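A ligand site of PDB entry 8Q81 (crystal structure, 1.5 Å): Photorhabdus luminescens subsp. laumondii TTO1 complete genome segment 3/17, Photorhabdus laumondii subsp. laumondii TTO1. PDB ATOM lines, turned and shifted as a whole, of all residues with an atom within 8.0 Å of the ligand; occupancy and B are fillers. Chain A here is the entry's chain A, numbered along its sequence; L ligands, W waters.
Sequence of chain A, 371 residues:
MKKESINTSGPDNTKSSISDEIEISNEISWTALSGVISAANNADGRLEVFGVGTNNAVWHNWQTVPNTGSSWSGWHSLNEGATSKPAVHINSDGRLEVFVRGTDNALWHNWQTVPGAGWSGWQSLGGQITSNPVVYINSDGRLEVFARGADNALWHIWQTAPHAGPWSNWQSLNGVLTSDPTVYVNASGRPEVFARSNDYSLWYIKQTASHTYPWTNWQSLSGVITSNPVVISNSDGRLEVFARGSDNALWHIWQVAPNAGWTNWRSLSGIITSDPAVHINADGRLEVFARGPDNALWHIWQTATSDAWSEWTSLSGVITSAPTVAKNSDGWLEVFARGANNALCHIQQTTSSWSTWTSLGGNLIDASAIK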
ATOM      1  N   TYR A 200     -22.681   5.480  23.067  1.00  0.00           N
ATOM      2  CA  TYR A 200     -22.366   4.490  24.085  1.00  0.00           C
ATOM      3  C   TYR A 200     -20.942   3.953  23.956  1.00  0.00           C
ATOM      4  O   TYR A 200     -20.593   2.986  24.626  1.00  0.00           O
ATOM      5  CB  TYR A 200     -23.323   3.321  24.191  1.00  0.00           C
ATOM      6  CG  TYR A 200     -24.714   3.741  24.605  1.00  0.00           C
ATOM      7  CD1 TYR A 200     -25.049   3.824  25.949  1.00  0.00           C
ATOM      8  CD2 TYR A 200     -25.656   4.165  23.678  1.00  0.00           C
ATOM      9  CE1 TYR A 200     -26.299   4.267  26.352  1.00  0.00           C
ATOM     10  CE2 TYR A 200     -26.911   4.591  24.054  1.00  0.00           C
ATOM     11  CZ  TYR A 200     -27.234   4.647  25.401  1.00  0.00           C
ATOM     12  OH  TYR A 200     -28.479   5.074  25.778  1.00  0.00           O
ATOM     13  N   SER A 201     -20.125   4.606  23.132  1.00  0.00           N
ATOM     14  CA  SER A 201     -18.730   4.242  22.964  1.00  0.00           C
ATOM     15  C   SER A 201     -17.839   5.078  23.862  1.00  0.00           C
ATOM     16  O   SER A 201     -18.236   6.124  24.353  1.00  0.00           O
ATOM     17  CB  SER A 201     -18.279   4.387  21.534  1.00  0.00           C
ATOM     18  OG  SER A 201     -18.868   3.401  20.660  1.00  0.00           O
ATOM     19  N   LEU A 202     -16.610   4.554  24.048  1.00  0.00           N
ATOM     20  CA  LEU A 202     -15.569   5.246  24.806  1.00  0.00           C
ATOM     21  C   LEU A 202     -14.819   6.198  23.865  1.00  0.00           C
ATOM     22  O   LEU A 202     -14.353   5.777  22.794  1.00  0.00           O
ATOM     23  CB  LEU A 202     -14.619   4.213  25.407  1.00  0.00           C
ATOM     24  CG  LEU A 202     -13.525   4.798  26.286  1.00  0.00           C
ATOM     25  CD1 LEU A 202     -14.100   5.330  27.578  1.00  0.00           C
ATOM     26  CD2 LEU A 202     -12.456   3.743  26.533  1.00  0.00           C
ATOM     27  N   LEU A 221     -12.628   5.060  20.787  1.00  0.00           N
ATOM     28  CA  LEU A 221     -12.174   3.690  20.972  1.00  0.00           C
ATOM     29  C   LEU A 221     -13.354   2.718  20.889  1.00  0.00           C
ATOM     30  O   LEU A 221     -13.207   1.519  21.228  1.00  0.00           O
ATOM     31  CB  LEU A 221     -11.499   3.606  22.345  1.00  0.00           C
ATOM     32  CG  LEU A 221     -10.130   4.274  22.469  1.00  0.00           C
ATOM     33  CD1 LEU A 221      -9.631   4.304  23.888  1.00  0.00           C
ATOM     34  CD2 LEU A 221      -9.187   3.515  21.589  1.00  0.00           C
ATOM     35  N   SER A 222     -14.482   3.184  20.356  1.00  0.00           N
ATOM     36  CA  SER A 222     -15.613   2.312  20.072  1.00  0.00           C
ATOM     37  C   SER A 222     -16.104   1.640  21.350  1.00  0.00           C
ATOM     38  O   SER A 222     -15.946   2.182  22.448  1.00  0.00           O
ATOM     39  CB  SER A 222     -15.271   1.277  18.994  1.00  0.00           C
ATOM     40  OG  SER A 222     -16.449   0.659  18.462  1.00  0.00           O
ATOM     41  N   GLY A 223     -16.713   0.464  21.196  1.00  0.00           N
ATOM     42  CA  GLY A 223     -17.289  -0.278  22.303  1.00  0.00           C
ATOM     43  C   GLY A 223     -18.749   0.105  22.574  1.00  0.00           C
ATOM     44  O   GLY A 223     -19.231   1.144  22.102  1.00  0.00           O
ATOM     45  N   VAL A 224     -19.390  -0.729  23.386  1.00  0.00           N
ATOM     46  CA  VAL A 224     -20.665  -0.434  23.990  1.00  0.00           C
ATOM     47  C   VAL A 224     -20.436  -0.587  25.486  1.00  0.00           C
ATOM     48  O   VAL A 224     -20.193  -1.684  25.958  1.00  0.00           O
ATOM     49  CB  VAL A 224     -21.807  -1.365  23.523  1.00  0.00           C
ATOM     50  CG1 VAL A 224     -23.117  -1.030  24.213  1.00  0.00           C
ATOM     51  CG2 VAL A 224     -21.943  -1.350  22.007  1.00  0.00           C
ATOM     52  N   ILE A 225     -20.494   0.522  26.211  1.00  0.00           N
ATOM     53  CA  ILE A 225     -20.246   0.365  27.638  1.00  0.00           C
ATOM     54  C   ILE A 225     -21.432   0.854  28.455  1.00  0.00           C
ATOM     55  O   ILE A 225     -22.170   1.763  28.079  1.00  0.00           O
ATOM     56  CB  ILE A 225     -18.899   0.970  28.051  1.00  0.00           C
ATOM     57  CG1 ILE A 225     -18.912   2.479  27.815  1.00  0.00           C
ATOM     58  CG2 ILE A 225     -17.682   0.293  27.416  1.00  0.00           C
ATOM     59  CD1 ILE A 225     -17.799   3.229  28.535  1.00  0.00           C
ATOM     60  N   THR A 226     -21.625   0.130  29.563  1.00  0.00           N
ATOM     61  CA  THR A 226     -22.780   0.276  30.417  1.00  0.00           C
ATOM     62  C   THR A 226     -22.430   0.604  31.872  1.00  0.00           C
ATOM     63  O   THR A 226     -23.251   0.405  32.769  1.00  0.00           O
ATOM     64  CB  THR A 226     -23.628  -0.992  30.366  1.00  0.00           C
ATOM     65  OG1 THR A 226     -22.876  -2.047  30.948  1.00  0.00           O
ATOM     66  CG2 THR A 226     -24.028  -1.392  28.952  1.00  0.00           C
ATOM     67  N   ALA A 243     -14.397  -1.110  31.844  1.00  0.00           N
ATOM     68  CA  ALA A 243     -15.799  -0.741  31.910  1.00  0.00           C
ATOM     69  C   ALA A 243     -16.663  -1.985  31.812  1.00  0.00           C
ATOM     70  O   ALA A 243     -16.239  -3.007  31.252  1.00  0.00           O
ATOM     71  CB  ALA A 243     -16.135   0.196  30.778  1.00  0.00           C
ATOM     72  N   ARG A 244     -17.898  -1.896  32.308  1.00  0.00           N
ATOM     73  CA  ARG A 244     -18.865  -2.948  32.039  1.00  0.00           C
ATOM     74  C   ARG A 244     -19.358  -2.893  30.600  1.00  0.00           C
ATOM     75  O   ARG A 244     -19.527  -1.807  30.031  1.00  0.00           O
ATOM     76  CB  ARG A 244     -20.077  -2.823  32.951  1.00  0.00           C
ATOM     77  CG  ARG A 244     -21.005  -4.029  32.934  1.00  0.00           C
ATOM     78  CD  ARG A 244     -22.039  -3.905  34.028  1.00  0.00           C
ATOM     79  NE  ARG A 244     -22.994  -2.825  33.824  1.00  0.00           N
ATOM     80  CZ  ARG A 244     -23.982  -2.551  34.641  1.00  0.00           C
ATOM     81  NH1 ARG A 244     -24.162  -3.283  35.730  1.00  0.00           N
ATOM     82  NH2 ARG A 244     -24.764  -1.515  34.371  1.00  0.00           N
ATOM     83  N   GLY A 245     -19.534  -4.084  30.013  1.00  0.00           N
ATOM     84  CA  GLY A 245     -19.983  -4.164  28.633  1.00  0.00           C
ATOM     85  C   GLY A 245     -21.468  -4.479  28.567  1.00  0.00           C
ATOM     86  O   GLY A 245     -22.130  -4.593  29.587  1.00  0.00           O
ATOM     87  N   SER A 246     -21.978  -4.664  27.330  1.00  0.00           N
ATOM     88  CA  SER A 246     -23.410  -4.822  27.152  1.00  0.00           C
ATOM     89  C   SER A 246     -23.898  -6.178  27.644  1.00  0.00           C
ATOM     90  O   SER A 246     -25.113  -6.387  27.778  1.00  0.00           O
ATOM     91  CB  SER A 246     -23.728  -4.602  25.682  1.00  0.00           C
ATOM     92  OG  SER A 246     -23.113  -5.602  24.889  1.00  0.00           O
ATOM     93  N   ASP A 247     -22.968  -7.121  27.884  1.00  0.00           N
ATOM     94  CA  ASP A 247     -23.245  -8.470  28.383  1.00  0.00           C
ATOM     95  C   ASP A 247     -22.985  -8.526  29.897  1.00  0.00           C
ATOM     96  O   ASP A 247     -23.040  -9.612  30.478  1.00  0.00           O
ATOM     97  CB  ASP A 247     -22.418  -9.498  27.607  1.00  0.00           C
ATOM     98  CG  ASP A 247     -20.913  -9.283  27.733  1.00  0.00           C
ATOM     99  OD1 ASP A 247     -20.515  -8.281  28.358  1.00  0.00           O
ATOM    100  OD2 ASP A 247     -20.136 -10.086  27.134  1.00  0.00           O
ATOM    101  N   ASN A 248     -22.750  -7.365  30.516  1.00  0.00           N
ATOM    102  CA  ASN A 248     -22.487  -7.193  31.949  1.00  0.00           C
ATOM    103  C   ASN A 248     -21.159  -7.773  32.411  1.00  0.00           C
ATOM    104  O   ASN A 248     -20.898  -7.833  33.618  1.00  0.00           O
ATOM    105  CB  ASN A 248     -23.644  -7.701  32.808  1.00  0.00           C
ATOM    106  CG  ASN A 248     -24.846  -6.817  32.671  1.00  0.00           C
ATOM    107  OD1 ASN A 248     -24.724  -5.602  32.733  1.00  0.00           O
ATOM    108  ND2 ASN A 248     -25.979  -7.437  32.418  1.00  0.00           N
ATOM    109  N   ALA A 249     -20.342  -8.239  31.470  1.00  0.00           N
ATOM    110  CA  ALA A 249     -18.972  -8.606  31.800  1.00  0.00           C
ATOM    111  C   ALA A 249     -18.131  -7.355  31.995  1.00  0.00           C
ATOM    112  O   ALA A 249     -18.469  -6.262  31.552  1.00  0.00           O
ATOM    113  CB  ALA A 249     -18.388  -9.504  30.723  1.00  0.00           C
ATOM    114  N   LEU A 250     -16.973  -7.576  32.621  1.00  0.00           N
ATOM    115  CA  LEU A 250     -15.916  -6.563  32.612  1.00  0.00           C
ATOM    116  C   LEU A 250     -15.162  -6.616  31.296  1.00  0.00           C
ATOM    117  O   LEU A 250     -14.642  -7.691  30.960  1.00  0.00           O
ATOM    118  CB  LEU A 250     -14.972  -6.868  33.760  1.00  0.00           C
ATOM    119  CG  LEU A 250     -13.744  -5.986  33.834  1.00  0.00           C
ATOM    120  CD1 LEU A 250     -14.129  -4.561  34.177  1.00  0.00           C
ATOM    121  CD2 LEU A 250     -12.735  -6.512  34.849  1.00  0.00           C
ATOM    122  N   TRP A 251     -15.046  -5.485  30.612  1.00  0.00           N
ATOM    123  CA  TRP A 251     -14.211  -5.380  29.438  1.00  0.00           C
ATOM    124  C   TRP A 251     -13.060  -4.412  29.661  1.00  0.00           C
ATOM    125  O   TRP A 251     -13.110  -3.607  30.574  1.00  0.00           O
ATOM    126  CB  TRP A 251     -15.065  -4.973  28.239  1.00  0.00           C
ATOM    127  CG  TRP A 251     -16.040  -6.032  27.804  1.00  0.00           C
ATOM    128  CD1 TRP A 251     -17.203  -6.434  28.411  1.00  0.00           C
ATOM    129  CD2 TRP A 251     -15.985  -6.743  26.562  1.00  0.00           C
ATOM    130  NE1 TRP A 251     -17.839  -7.371  27.642  1.00  0.00           N
ATOM    131  CE2 TRP A 251     -17.107  -7.602  26.514  1.00  0.00           C
ATOM    132  CE3 TRP A 251     -15.076  -6.744  25.499  1.00  0.00           C
ATOM    133  CZ2 TRP A 251     -17.345  -8.447  25.428  1.00  0.00           C
ATOM    134  CZ3 TRP A 251     -15.314  -7.569  24.404  1.00  0.00           C
ATOM    135  CH2 TRP A 251     -16.472  -8.359  24.360  1.00  0.00           C
ATOM    136  N   HIS A 252     -12.024  -4.492  28.828  1.00  0.00           N
ATOM    137  CA  HIS A 252     -10.875  -3.623  28.979  1.00  0.00           C
ATOM    138  C   HIS A 252     -10.223  -3.439  27.609  1.00  0.00           C
ATOM    139  O   HIS A 252     -10.456  -4.187  26.660  1.00  0.00           O
ATOM    140  CB  HIS A 252      -9.878  -4.082  30.038  1.00  0.00           C
ATOM    141  CG  HIS A 252      -9.104  -5.324  29.721  1.00  0.00           C
ATOM    142  ND1 HIS A 252      -7.760  -5.453  30.030  1.00  0.00           N
ATOM    143  CD2 HIS A 252      -9.455  -6.477  29.128  1.00  0.00           C
ATOM    144  CE1 HIS A 252      -7.343  -6.674  29.641  1.00  0.00           C
ATOM    145  NE2 HIS A 252      -8.349  -7.329  29.129  1.00  0.00           N
ATOM    146  N   ILE A 253      -9.446  -2.363  27.543  1.00  0.00           N
ATOM    147  CA  ILE A 253      -8.770  -1.958  26.325  1.00  0.00           C
ATOM    148  C   ILE A 253      -7.496  -1.269  26.778  1.00  0.00           C
ATOM    149  O   ILE A 253      -7.543  -0.602  27.824  1.00  0.00           O
ATOM    150  CB  ILE A 253      -9.706  -1.066  25.472  1.00  0.00           C
ATOM    151  CG1 ILE A 253      -9.102  -0.765  24.094  1.00  0.00           C
ATOM    152  CG2 ILE A 253     -10.100   0.185  26.205  1.00  0.00           C
ATOM    153  CD1 ILE A 253     -10.098  -0.200  23.113  1.00  0.00           C
ATOM    154  N   ASN A 264      -7.947  -3.769  20.582  1.00  0.00           N
ATOM    155  CA  ASN A 264      -9.392  -3.872  20.556  1.00  0.00           C
ATOM    156  C   ASN A 264      -9.901  -4.083  22.005  1.00  0.00           C
ATOM    157  O   ASN A 264      -9.162  -4.384  22.944  1.00  0.00           O
ATOM    158  CB  ASN A 264      -9.808  -4.988  19.594  1.00  0.00           C
ATOM    159  CG  ASN A 264      -9.365  -6.367  20.022  1.00  0.00           C
ATOM    160  OD1 ASN A 264      -8.264  -6.567  20.532  1.00  0.00           O
ATOM    161  ND2 ASN A 264     -10.225  -7.357  19.827  1.00  0.00           N
ATOM    162  N   TRP A 265     -11.224  -3.971  22.158  1.00  0.00           N
ATOM    163  CA  TRP A 265     -11.867  -4.322  23.398  1.00  0.00           C
ATOM    164  C   TRP A 265     -11.832  -5.823  23.615  1.00  0.00           C
ATOM    165  O   TRP A 265     -12.085  -6.600  22.679  1.00  0.00           O
ATOM    166  CB  TRP A 265     -13.338  -3.883  23.414  1.00  0.00           C
ATOM    167  CG  TRP A 265     -13.551  -2.426  23.649  1.00  0.00           C
ATOM    168  CD1 TRP A 265     -13.784  -1.453  22.714  1.00  0.00           C
ATOM    169  CD2 TRP A 265     -13.565  -1.788  24.923  1.00  0.00           C
ATOM    170  NE1 TRP A 265     -13.926  -0.258  23.336  1.00  0.00           N
ATOM    171  CE2 TRP A 265     -13.799  -0.429  24.690  1.00  0.00           C
ATOM    172  CE3 TRP A 265     -13.392  -2.229  26.247  1.00  0.00           C
ATOM    173  CZ2 TRP A 265     -13.872   0.484  25.722  1.00  0.00           C
ATOM    174  CZ3 TRP A 265     -13.503  -1.340  27.268  1.00  0.00           C
ATOM    175  CH2 TRP A 265     -13.704   0.012  27.018  1.00  0.00           C
ATOM    176  N   ARG A 266     -11.518  -6.241  24.848  1.00  0.00           N
ATOM    177  CA  ARG A 266     -11.397  -7.640  25.198  1.00  0.00           C
ATOM    178  C   ARG A 266     -12.128  -7.898  26.512  1.00  0.00           C
ATOM    179  O   ARG A 266     -12.159  -7.030  27.402  1.00  0.00           O
ATOM    180  CB  ARG A 266      -9.932  -8.050  25.286  1.00  0.00           C
ATOM    181  CG  ARG A 266      -9.243  -7.874  23.951  1.00  0.00           C
ATOM    182  CD  ARG A 266      -7.950  -8.650  23.871  1.00  0.00           C
ATOM    183  NE  ARG A 266      -7.236  -8.221  22.664  1.00  0.00           N
ATOM    184  CZ  ARG A 266      -5.950  -8.479  22.488  1.00  0.00           C
ATOM    185  NH1 ARG A 266      -5.347  -9.365  23.259  1.00  0.00           N
ATOM    186  NH2 ARG A 266      -5.312  -7.851  21.512  1.00  0.00           N
ATOM    187  N   SER A 267     -12.777  -9.051  26.573  1.00  0.00           N
ATOM    188  CA  SER A 267     -13.573  -9.403  27.749  1.00  0.00           C
ATOM    189  C   SER A 267     -12.728 -10.100  28.804  1.00  0.00           C
ATOM    190  O   SER A 267     -11.960 -11.042  28.507  1.00  0.00           O
ATOM    191  CB  SER A 267     -14.752 -10.251  27.364  1.00  0.00           C
ATOM    192  OG  SER A 267     -15.548 -10.570  28.516  1.00  0.00           O
HETATM  193  C1  LIG L   1     -18.654  -4.175  22.161  1.00  0.00           C
HETATM  194  C2  LIG L   1     -19.830  -5.059  22.537  1.00  0.00           C
HETATM  195  C3  LIG L   1     -19.494  -5.942  23.715  1.00  0.00           C
HETATM  196  C4  LIG L   1     -18.983  -5.080  24.874  1.00  0.00           C
HETATM  197  C5  LIG L   1     -17.800  -4.260  24.403  1.00  0.00           C
HETATM  198  C6  LIG L   1     -17.239  -3.306  25.433  1.00  0.00           C
HETATM  199  O1  LIG L   1     -17.663  -5.013  21.651  1.00  0.00           O
HETATM  200  O2  LIG L   1     -20.197  -5.852  21.408  1.00  0.00           O
HETATM  201  O3  LIG L   1     -20.629  -6.675  24.158  1.00  0.00           O
HETATM  202  O4  LIG L   1     -20.078  -4.299  25.367  1.00  0.00           O
HETATM  203  O5  LIG L   1     -18.203  -3.425  23.298  1.00  0.00           O
HETATM  204  C7  LIG L   1     -16.586  -4.298  21.123  1.00  0.00           C
HETATM  205  O   HOH W   1     -22.717  -5.012  20.470  1.00  0.00           O
HETATM  206  O   HOH W   2     -18.465  -7.189  19.620  1.00  0.00           O
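OG of Ser 201 lies within hydrogen-bond range of O of Gly 223 (2.7 Å). The indole nitrogen (NE1) of Trp 265 sits at hydrogen-bond distance from the backbone carbonyl oxygen (O) of Leu 221. The backbone NH (N) of Trp 251 lies within hydrogen-bond range of the backbone carbonyl oxygen (O) of Ala 243 (2.8 Å). NE1 of Trp 251 is in hydrogen-bond range of OD1 of Asp 247, at 2.9 Å. The backbone carbonyl oxygen (O) of Ser 222 sits at hydrogen-bond distance from the indole nitrogen (NE1) of Trp 265. The backbone carbonyl oxygen (O) of Gly 245 is in hydrogen-bond range of the side-chain hydroxyl (OG1) of Thr 226 (3.0 Å).
Gly 223 touches the ligand (CA to O5, 3.4 Å). CA of Gly 245 touches O4 of the ligand, 3.3 Å away. Trp 251 touches the ligand (CE2 to C4, 3.5 Å). Trp 265 touches the ligand (CB to C7, 3.996 Å). Hydrophobic or aromatic side chains within 4 Å of the ligand: Val 224, Trp 251 and Trp 265. The nearest printed residue that does not touch the ligand is Ile 225 (4.1 Å).
The side-chain hydroxyl of Ser 246 lies within hydrogen-bond range of an oxygen (O3) of the ligand. The backbone NH (N) of Val 224 lies within hydrogen-bond range of an oxygen (O5) of the ligand (2.9 Å). The backbone NH of Ser 246 is in hydrogen-bond range of an oxygen (O4) of the ligand, 2.8 Å away. The backbone carbonyl oxygen of Val 224 sits at hydrogen-bond distance from an oxygen (O4) of the ligand (2.7 Å).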
